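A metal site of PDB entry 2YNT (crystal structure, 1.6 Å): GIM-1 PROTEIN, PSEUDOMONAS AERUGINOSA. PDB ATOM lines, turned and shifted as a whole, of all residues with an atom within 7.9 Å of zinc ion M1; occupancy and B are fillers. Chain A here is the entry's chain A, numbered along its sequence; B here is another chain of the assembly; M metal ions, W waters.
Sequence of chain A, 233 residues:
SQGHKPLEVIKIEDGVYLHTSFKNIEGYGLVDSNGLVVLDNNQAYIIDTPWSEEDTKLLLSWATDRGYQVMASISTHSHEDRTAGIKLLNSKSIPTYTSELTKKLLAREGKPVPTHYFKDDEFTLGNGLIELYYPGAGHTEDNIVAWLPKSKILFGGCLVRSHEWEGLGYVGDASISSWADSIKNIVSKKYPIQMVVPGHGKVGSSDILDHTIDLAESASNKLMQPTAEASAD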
ATOM      1  N   ASP A  32     -26.933  16.628 -12.070  1.00  0.00           N
ATOM      2  CA  ASP A  32     -27.833  17.484 -12.836  1.00  0.00           C
ATOM      3  C   ASP A  32     -27.401  17.587 -14.284  1.00  0.00           C
ATOM      4  O   ASP A  32     -26.249  17.303 -14.624  1.00  0.00           O
ATOM      5  CB  ASP A  32     -27.823  18.891 -12.233  1.00  0.00           C
ATOM      6  CG  ASP A  32     -26.468  19.574 -12.389  1.00  0.00           C
ATOM      7  OD1 ASP A  32     -25.518  19.169 -11.673  1.00  0.00           O
ATOM      8  OD2 ASP A  32     -26.353  20.499 -13.223  1.00  0.00           O
ATOM      9  N   SER A  33     -28.336  18.035 -15.128  1.00  0.00           N
ATOM     10  CA  SER A  33     -28.081  18.269 -16.547  1.00  0.00           C
ATOM     11  C   SER A  33     -28.924  19.463 -17.009  1.00  0.00           C
ATOM     12  O   SER A  33     -30.138  19.510 -16.727  1.00  0.00           O
ATOM     13  CB  SER A  33     -28.437  17.015 -17.350  1.00  0.00           C
ATOM     14  OG  SER A  33     -28.240  17.210 -18.734  1.00  0.00           O
ATOM     15  N   ASN A  34     -28.313  20.410 -17.714  1.00  0.00           N
ATOM     16  CA  ASN A  34     -28.979  21.661 -18.115  1.00  0.00           C
ATOM     17  C   ASN A  34     -29.231  21.781 -19.597  1.00  0.00           C
ATOM     18  O   ASN A  34     -28.422  21.336 -20.423  1.00  0.00           O
ATOM     19  CB  ASN A  34     -28.097  22.877 -17.784  1.00  0.00           C
ATOM     20  CG  ASN A  34     -27.790  22.995 -16.324  1.00  0.00           C
ATOM     21  OD1 ASN A  34     -28.659  22.878 -15.461  1.00  0.00           O
ATOM     22  ND2 ASN A  34     -26.510  23.236 -16.023  1.00  0.00           N
ATOM     23  N   ASP A  48     -31.256  21.554 -26.176  1.00  0.00           N
ATOM     24  CA  ASP A  48     -31.109  20.275 -25.487  1.00  0.00           C
ATOM     25  C   ASP A  48     -32.347  19.811 -24.740  1.00  0.00           C
ATOM     26  O   ASP A  48     -33.027  20.600 -24.071  1.00  0.00           O
ATOM     27  CB  ASP A  48     -29.846  20.245 -24.597  1.00  0.00           C
ATOM     28  CG  ASP A  48     -28.581  20.181 -25.431  1.00  0.00           C
ATOM     29  OD1 ASP A  48     -28.593  19.497 -26.471  1.00  0.00           O
ATOM     30  OD2 ASP A  48     -27.569  20.803 -25.037  1.00  0.00           O
ATOM     31  N   TRP A  51     -33.075  15.060 -19.462  1.00  0.00           N
ATOM     32  CA  TRP A  51     -32.381  13.772 -19.440  1.00  0.00           C
ATOM     33  C   TRP A  51     -33.305  12.549 -19.526  1.00  0.00           C
ATOM     34  O   TRP A  51     -32.830  11.412 -19.619  1.00  0.00           O
ATOM     35  CB  TRP A  51     -31.547  13.725 -18.157  1.00  0.00           C
ATOM     36  CG  TRP A  51     -30.294  12.904 -18.194  1.00  0.00           C
ATOM     37  CD1 TRP A  51     -29.957  11.907 -19.074  1.00  0.00           C
ATOM     38  CD2 TRP A  51     -29.188  13.015 -17.287  1.00  0.00           C
ATOM     39  NE1 TRP A  51     -28.711  11.391 -18.750  1.00  0.00           N
ATOM     40  CE2 TRP A  51     -28.221  12.061 -17.661  1.00  0.00           C
ATOM     41  CE3 TRP A  51     -28.940  13.836 -16.181  1.00  0.00           C
ATOM     42  CZ2 TRP A  51     -27.004  11.919 -16.975  1.00  0.00           C
ATOM     43  CZ3 TRP A  51     -27.735  13.688 -15.500  1.00  0.00           C
ATOM     44  CH2 TRP A  51     -26.775  12.745 -15.908  1.00  0.00           C
ATOM     45  N   THR A  76     -27.121  19.264 -28.730  1.00  0.00           N
ATOM     46  CA  THR A  76     -25.756  19.751 -28.918  1.00  0.00           C
ATOM     47  C   THR A  76     -24.671  18.669 -28.984  1.00  0.00           C
ATOM     48  O   THR A  76     -23.525  18.979 -29.261  1.00  0.00           O
ATOM     49  CB  THR A  76     -25.380  20.839 -27.886  1.00  0.00           C
ATOM     50  OG1 THR A  76     -25.468  20.331 -26.548  1.00  0.00           O
ATOM     51  CG2 THR A  76     -26.315  22.034 -28.045  1.00  0.00           C
ATOM     52  N   HIS A  77     -25.039  17.422 -28.673  1.00  0.00           N
ATOM     53  CA  HIS A  77     -24.290  16.229 -29.071  1.00  0.00           C
ATOM     54  C   HIS A  77     -25.175  15.013 -28.877  1.00  0.00           C
ATOM     55  O   HIS A  77     -26.322  15.149 -28.475  1.00  0.00           O
ATOM     56  CB  HIS A  77     -22.903  16.105 -28.410  1.00  0.00           C
ATOM     57  CG  HIS A  77     -22.913  15.982 -26.915  1.00  0.00           C
ATOM     58  ND1 HIS A  77     -23.102  17.049 -26.072  1.00  0.00           N
ATOM     59  CD2 HIS A  77     -22.714  14.903 -26.113  1.00  0.00           C
ATOM     60  CE1 HIS A  77     -23.013  16.649 -24.818  1.00  0.00           C
ATOM     61  NE2 HIS A  77     -22.784  15.352 -24.811  1.00  0.00           N
ATOM     62  N   HIS A  79     -25.107  12.339 -26.857  1.00  0.00           N
ATOM     63  CA  HIS A  79     -25.335  11.714 -25.554  1.00  0.00           C
ATOM     64  C   HIS A  79     -26.785  11.827 -25.071  1.00  0.00           C
ATOM     65  O   HIS A  79     -27.496  12.790 -25.401  1.00  0.00           O
ATOM     66  CB  HIS A  79     -24.415  12.317 -24.489  1.00  0.00           C
ATOM     67  CG  HIS A  79     -23.006  11.819 -24.556  1.00  0.00           C
ATOM     68  ND1 HIS A  79     -21.964  12.473 -23.925  1.00  0.00           N
ATOM     69  CD2 HIS A  79     -22.456  10.730 -25.147  1.00  0.00           C
ATOM     70  CE1 HIS A  79     -20.838  11.794 -24.129  1.00  0.00           C
ATOM     71  NE2 HIS A  79     -21.116  10.736 -24.864  1.00  0.00           N
ATOM     72  N   GLU A  80     -27.187  10.842 -24.266  1.00  0.00           N
ATOM     73  CA  GLU A  80     -28.537  10.754 -23.724  1.00  0.00           C
ATOM     74  C   GLU A  80     -29.004  12.036 -23.021  1.00  0.00           C
ATOM     75  O   GLU A  80     -30.157  12.432 -23.153  1.00  0.00           O
ATOM     76  CB  GLU A  80     -28.634   9.545 -22.771  1.00  0.00           C
ATOM     77  CG  GLU A  80     -30.033   9.270 -22.208  1.00  0.00           C
ATOM     78  CD  GLU A  80     -30.992   8.672 -23.222  1.00  0.00           C
ATOM     79  OE1 GLU A  80     -30.563   8.414 -24.376  1.00  0.00           O
ATOM     80  OE2 GLU A  80     -32.179   8.447 -22.869  1.00  0.00           O
ATOM     81  N   ASP A  81     -28.109  12.680 -22.265  1.00  0.00           N
ATOM     82  CA  ASP A  81     -28.519  13.865 -21.534  1.00  0.00           C
ATOM     83  C   ASP A  81     -28.855  15.059 -22.436  1.00  0.00           C
ATOM     84  O   ASP A  81     -29.442  16.030 -21.958  1.00  0.00           O
ATOM     85  CB  ASP A  81     -27.506  14.263 -20.425  1.00  0.00           C
ATOM     86  CG  ASP A  81     -26.088  14.445 -20.943  1.00  0.00           C
ATOM     87  OD1 ASP A  81     -25.455  13.455 -21.351  1.00  0.00           O
ATOM     88  OD2 ASP A  81     -25.566  15.596 -20.859  1.00  0.00           O
ATOM     89  N   ARG A  82     -28.504  14.972 -23.710  1.00  0.00           N
ATOM     90  CA  ARG A  82     -28.849  15.998 -24.691  1.00  0.00           C
ATOM     91  C   ARG A  82     -30.059  15.624 -25.558  1.00  0.00           C
ATOM     92  O   ARG A  82     -30.690  16.502 -26.145  1.00  0.00           O
ATOM     93  CB  ARG A  82     -27.694  16.257 -25.663  1.00  0.00           C
ATOM     94  CG  ARG A  82     -26.342  16.515 -25.034  1.00  0.00           C
ATOM     95  CD  ARG A  82     -26.316  17.832 -24.277  1.00  0.00           C
ATOM     96  NE  ARG A  82     -26.483  17.655 -22.833  1.00  0.00           N
ATOM     97  CZ  ARG A  82     -26.785  18.645 -21.996  1.00  0.00           C
ATOM     98  NH1 ARG A  82     -27.044  19.855 -22.458  1.00  0.00           N
ATOM     99  NH2 ARG A  82     -26.882  18.404 -20.689  1.00  0.00           N
ATOM    100  N   HIS A 139     -15.348  17.431 -25.448  1.00  0.00           N
ATOM    101  CA  HIS A 139     -16.128  16.518 -24.641  1.00  0.00           C
ATOM    102  C   HIS A 139     -16.556  15.311 -25.476  1.00  0.00           C
ATOM    103  O   HIS A 139     -16.488  14.159 -25.015  1.00  0.00           O
ATOM    104  CB  HIS A 139     -17.355  17.243 -24.064  1.00  0.00           C
ATOM    105  CG  HIS A 139     -18.389  16.321 -23.494  1.00  0.00           C
ATOM    106  ND1 HIS A 139     -18.229  15.709 -22.271  1.00  0.00           N
ATOM    107  CD2 HIS A 139     -19.580  15.897 -23.979  1.00  0.00           C
ATOM    108  CE1 HIS A 139     -19.281  14.935 -22.020  1.00  0.00           C
ATOM    109  NE2 HIS A 139     -20.117  15.046 -23.040  1.00  0.00           N
ATOM    110  N   THR A 140     -16.998  15.586 -26.700  1.00  0.00           N
ATOM    111  CA  THR A 140     -17.250  14.542 -27.695  1.00  0.00           C
ATOM    112  C   THR A 140     -16.770  15.052 -29.038  1.00  0.00           C
ATOM    113  O   THR A 140     -16.396  16.220 -29.185  1.00  0.00           O
ATOM    114  CB  THR A 140     -18.737  14.188 -27.828  1.00  0.00           C
ATOM    115  OG1 THR A 140     -19.484  15.392 -28.073  1.00  0.00           O
ATOM    116  CG2 THR A 140     -19.252  13.496 -26.566  1.00  0.00           C
ATOM    117  N   GLY A 157     -22.827  23.923 -23.357  1.00  0.00           N
ATOM    118  CA  GLY A 157     -23.117  22.501 -23.288  1.00  0.00           C
ATOM    119  C   GLY A 157     -22.024  21.781 -22.528  1.00  0.00           C
ATOM    120  O   GLY A 157     -21.336  22.364 -21.681  1.00  0.00           O
ATOM    121  N   CYS A 158     -21.854  20.512 -22.836  1.00  0.00           N
ATOM    122  CA  CYS A 158     -20.978  19.670 -22.022  1.00  0.00           C
ATOM    123  C   CYS A 158     -19.517  19.839 -22.416  1.00  0.00           C
ATOM    124  O   CYS A 158     -18.632  19.317 -21.759  1.00  0.00           O
ATOM    125  CB  CYS A 158     -21.441  18.230 -22.081  1.00  0.00           C
ATOM    126  SG  CYS A 158     -23.219  18.130 -21.694  1.00  0.00           S
ATOM    127  N   LEU A 159     -19.282  20.628 -23.478  1.00  0.00           N
ATOM    128  CA  LEU A 159     -17.916  20.995 -23.885  1.00  0.00           C
ATOM    129  C   LEU A 159     -17.271  21.923 -22.860  1.00  0.00           C
ATOM    130  O   LEU A 159     -16.047  21.959 -22.729  1.00  0.00           O
ATOM    131  CB  LEU A 159     -17.968  21.676 -25.258  1.00  0.00           C
ATOM    132  CG  LEU A 159     -16.670  22.291 -25.801  1.00  0.00           C
ATOM    133  CD1 LEU A 159     -15.612  21.192 -25.935  1.00  0.00           C
ATOM    134  CD2 LEU A 159     -16.937  22.929 -27.138  1.00  0.00           C
ATOM    135  N   ARG A 161     -16.870  23.263 -18.827  1.00  0.00           N
ATOM    136  CA  ARG A 161     -16.996  22.759 -17.471  1.00  0.00           C
ATOM    137  C   ARG A 161     -17.267  23.868 -16.478  1.00  0.00           C
ATOM    138  O   ARG A 161     -16.547  24.883 -16.426  1.00  0.00           O
ATOM    139  CB  ARG A 161     -15.719  21.989 -17.072  1.00  0.00           C
ATOM    140  CG  ARG A 161     -15.428  20.782 -17.965  1.00  0.00           C
ATOM    141  CD  ARG A 161     -16.444  19.665 -17.740  1.00  0.00           C
ATOM    142  NE  ARG A 161     -16.323  19.068 -16.422  1.00  0.00           N
ATOM    143  CZ  ARG A 161     -17.225  18.249 -15.877  1.00  0.00           C
ATOM    144  NH1 ARG A 161     -18.344  17.954 -16.539  1.00  0.00           N
ATOM    145  NH2 ARG A 161     -17.021  17.749 -14.671  1.00  0.00           N
ATOM    146  N   TYR A 170     -17.054  13.037 -17.612  1.00  0.00           N
ATOM    147  CA  TYR A 170     -16.985  11.826 -18.409  1.00  0.00           C
ATOM    148  C   TYR A 170     -16.207  12.056 -19.704  1.00  0.00           C
ATOM    149  O   TYR A 170     -16.592  12.898 -20.526  1.00  0.00           O
ATOM    150  CB  TYR A 170     -18.392  11.309 -18.715  1.00  0.00           C
ATOM    151  CG  TYR A 170     -18.385  10.086 -19.605  1.00  0.00           C
ATOM    152  CD1 TYR A 170     -18.056   8.843 -19.088  1.00  0.00           C
ATOM    153  CD2 TYR A 170     -18.715  10.168 -20.961  1.00  0.00           C
ATOM    154  CE1 TYR A 170     -18.040   7.708 -19.882  1.00  0.00           C
ATOM    155  CE2 TYR A 170     -18.704   9.038 -21.768  1.00  0.00           C
ATOM    156  CZ  TYR A 170     -18.364   7.802 -21.211  1.00  0.00           C
ATOM    157  OH  TYR A 170     -18.341   6.656 -21.972  1.00  0.00           O
ATOM    158  N   PRO A 198     -23.224  25.800 -18.792  1.00  0.00           N
ATOM    159  CA  PRO A 198     -22.621  24.479 -18.988  1.00  0.00           C
ATOM    160  C   PRO A 198     -23.704  23.405 -19.046  1.00  0.00           C
ATOM    161  O   PRO A 198     -24.822  23.646 -18.590  1.00  0.00           O
ATOM    162  CB  PRO A 198     -21.774  24.302 -17.746  1.00  0.00           C
ATOM    163  CG  PRO A 198     -22.551  24.997 -16.664  1.00  0.00           C
ATOM    164  CD  PRO A 198     -23.255  26.169 -17.358  1.00  0.00           C
ATOM    165  N   GLY A 199     -23.376  22.245 -19.609  1.00  0.00           N
ATOM    166  CA  GLY A 199     -24.320  21.142 -19.648  1.00  0.00           C
ATOM    167  C   GLY A 199     -24.578  20.527 -18.278  1.00  0.00           C
ATOM    168  O   GLY A 199     -25.626  19.916 -18.039  1.00  0.00           O
ATOM    169  N   HIS A 200     -23.606  20.662 -17.377  1.00  0.00           N
ATOM    170  CA  HIS A 200     -23.724  20.115 -16.026  1.00  0.00           C
ATOM    171  C   HIS A 200     -23.120  21.123 -15.058  1.00  0.00           C
ATOM    172  O   HIS A 200     -22.003  21.580 -15.265  1.00  0.00           O
ATOM    173  CB  HIS A 200     -22.971  18.789 -15.921  1.00  0.00           C
ATOM    174  CG  HIS A 200     -23.402  17.768 -16.919  1.00  0.00           C
ATOM    175  ND1 HIS A 200     -24.517  16.990 -16.748  1.00  0.00           N
ATOM    176  CD2 HIS A 200     -22.881  17.405 -18.121  1.00  0.00           C
ATOM    177  CE1 HIS A 200     -24.677  16.194 -17.793  1.00  0.00           C
ATOM    178  NE2 HIS A 200     -23.703  16.431 -18.645  1.00  0.00           N
ATOM    179  N   GLU B  26     -21.431   8.039 -18.186  1.00  0.00           N
ATOM    180  CA  GLU B  26     -21.899   9.259 -18.841  1.00  0.00           C
ATOM    181  C   GLU B  26     -22.631  10.198 -17.903  1.00  0.00           C
ATOM    182  O   GLU B  26     -23.446   9.771 -17.087  1.00  0.00           O
ATOM    183  CB  GLU B  26     -22.847   8.911 -19.991  1.00  0.00           C
ATOM    184  CG  GLU B  26     -22.148   8.489 -21.252  1.00  0.00           C
ATOM    185  CD  GLU B  26     -23.107   8.360 -22.410  1.00  0.00           C
ATOM    186  OE1 GLU B  26     -24.093   9.129 -22.460  1.00  0.00           O
ATOM    187  OE2 GLU B  26     -22.867   7.488 -23.273  1.00  0.00           O
ATOM    188  N   GLY B  27     -22.367  11.499 -18.049  1.00  0.00           N
ATOM    189  CA  GLY B  27     -22.991  12.493 -17.210  1.00  0.00           C
ATOM    190  C   GLY B  27     -22.192  12.821 -15.971  1.00  0.00           C
ATOM    191  O   GLY B  27     -22.450  13.829 -15.310  1.00  0.00           O
ATOM    192  N   TYR B  28     -21.204  11.973 -15.650  1.00  0.00           N
ATOM    193  CA  TYR B  28     -20.404  12.194 -14.452  1.00  0.00           C
ATOM    194  C   TYR B  28     -18.904  11.896 -14.588  1.00  0.00           C
ATOM    195  O   TYR B  28     -18.082  12.750 -14.283  1.00  0.00           O
ATOM    196  CB  TYR B  28     -20.989  11.431 -13.253  1.00  0.00           C
ATOM    197  CG  TYR B  28     -20.114  11.573 -12.029  1.00  0.00           C
ATOM    198  CD1 TYR B  28     -20.144  12.731 -11.269  1.00  0.00           C
ATOM    199  CD2 TYR B  28     -19.241  10.554 -11.643  1.00  0.00           C
ATOM    200  CE1 TYR B  28     -19.339  12.880 -10.159  1.00  0.00           C
ATOM    201  CE2 TYR B  28     -18.429  10.690 -10.533  1.00  0.00           C
ATOM    202  CZ  TYR B  28     -18.487  11.864  -9.804  1.00  0.00           C
ATOM    203  OH  TYR B  28     -17.691  12.016  -8.697  1.00  0.00           O
HETATM  204 ZN    ZN M   1     -23.626  16.130 -20.695  1.00  0.00          ZN
HETATM  205 ZN    ZN M   2     -22.009  14.320 -23.208  1.00  0.00          ZN
HETATM  206  O   HOH W   1     -22.860  14.396 -21.459  1.00  0.00           O
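Zinc ion M1 is bound by the side-chain carboxylate (OD2) of Asp 81 (2.0 Å), water W1 (2.0 Å), a ring nitrogen (NE2) of His 200 (2.1 Å) and the side-chain sulfur (SG) of Cys 158 (2.3 Å).
Zinc ion M1 has four donor atoms within binding distance.
NE of Arg 82 touches zinc ion M1, 3.9 Å away.
OD2 of Asp 81 lies close to NE of Arg 82, at 3.0 Å.
ND1 of His 200 sits at hydrogen-bond distance from O of Asp 32 (2.8 Å).
The guanidinium group of Arg 82 lies close to the side-chain sulfur of Cys 158 (3.5 Å).
O of Gly 199 lies within hydrogen-bond range of NH2 of Arg 82 (3.3 Å).
OG of Ser 33 sits at hydrogen-bond distance from NH2 of Arg 82 (2.7 Å).
NH1 of Arg 82 is in hydrogen-bond range of O of Asn 34 (2.9 Å).
NH1 of Arg 82 is in salt-bridge range of OD2 of Asp 48 (2.8 Å).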
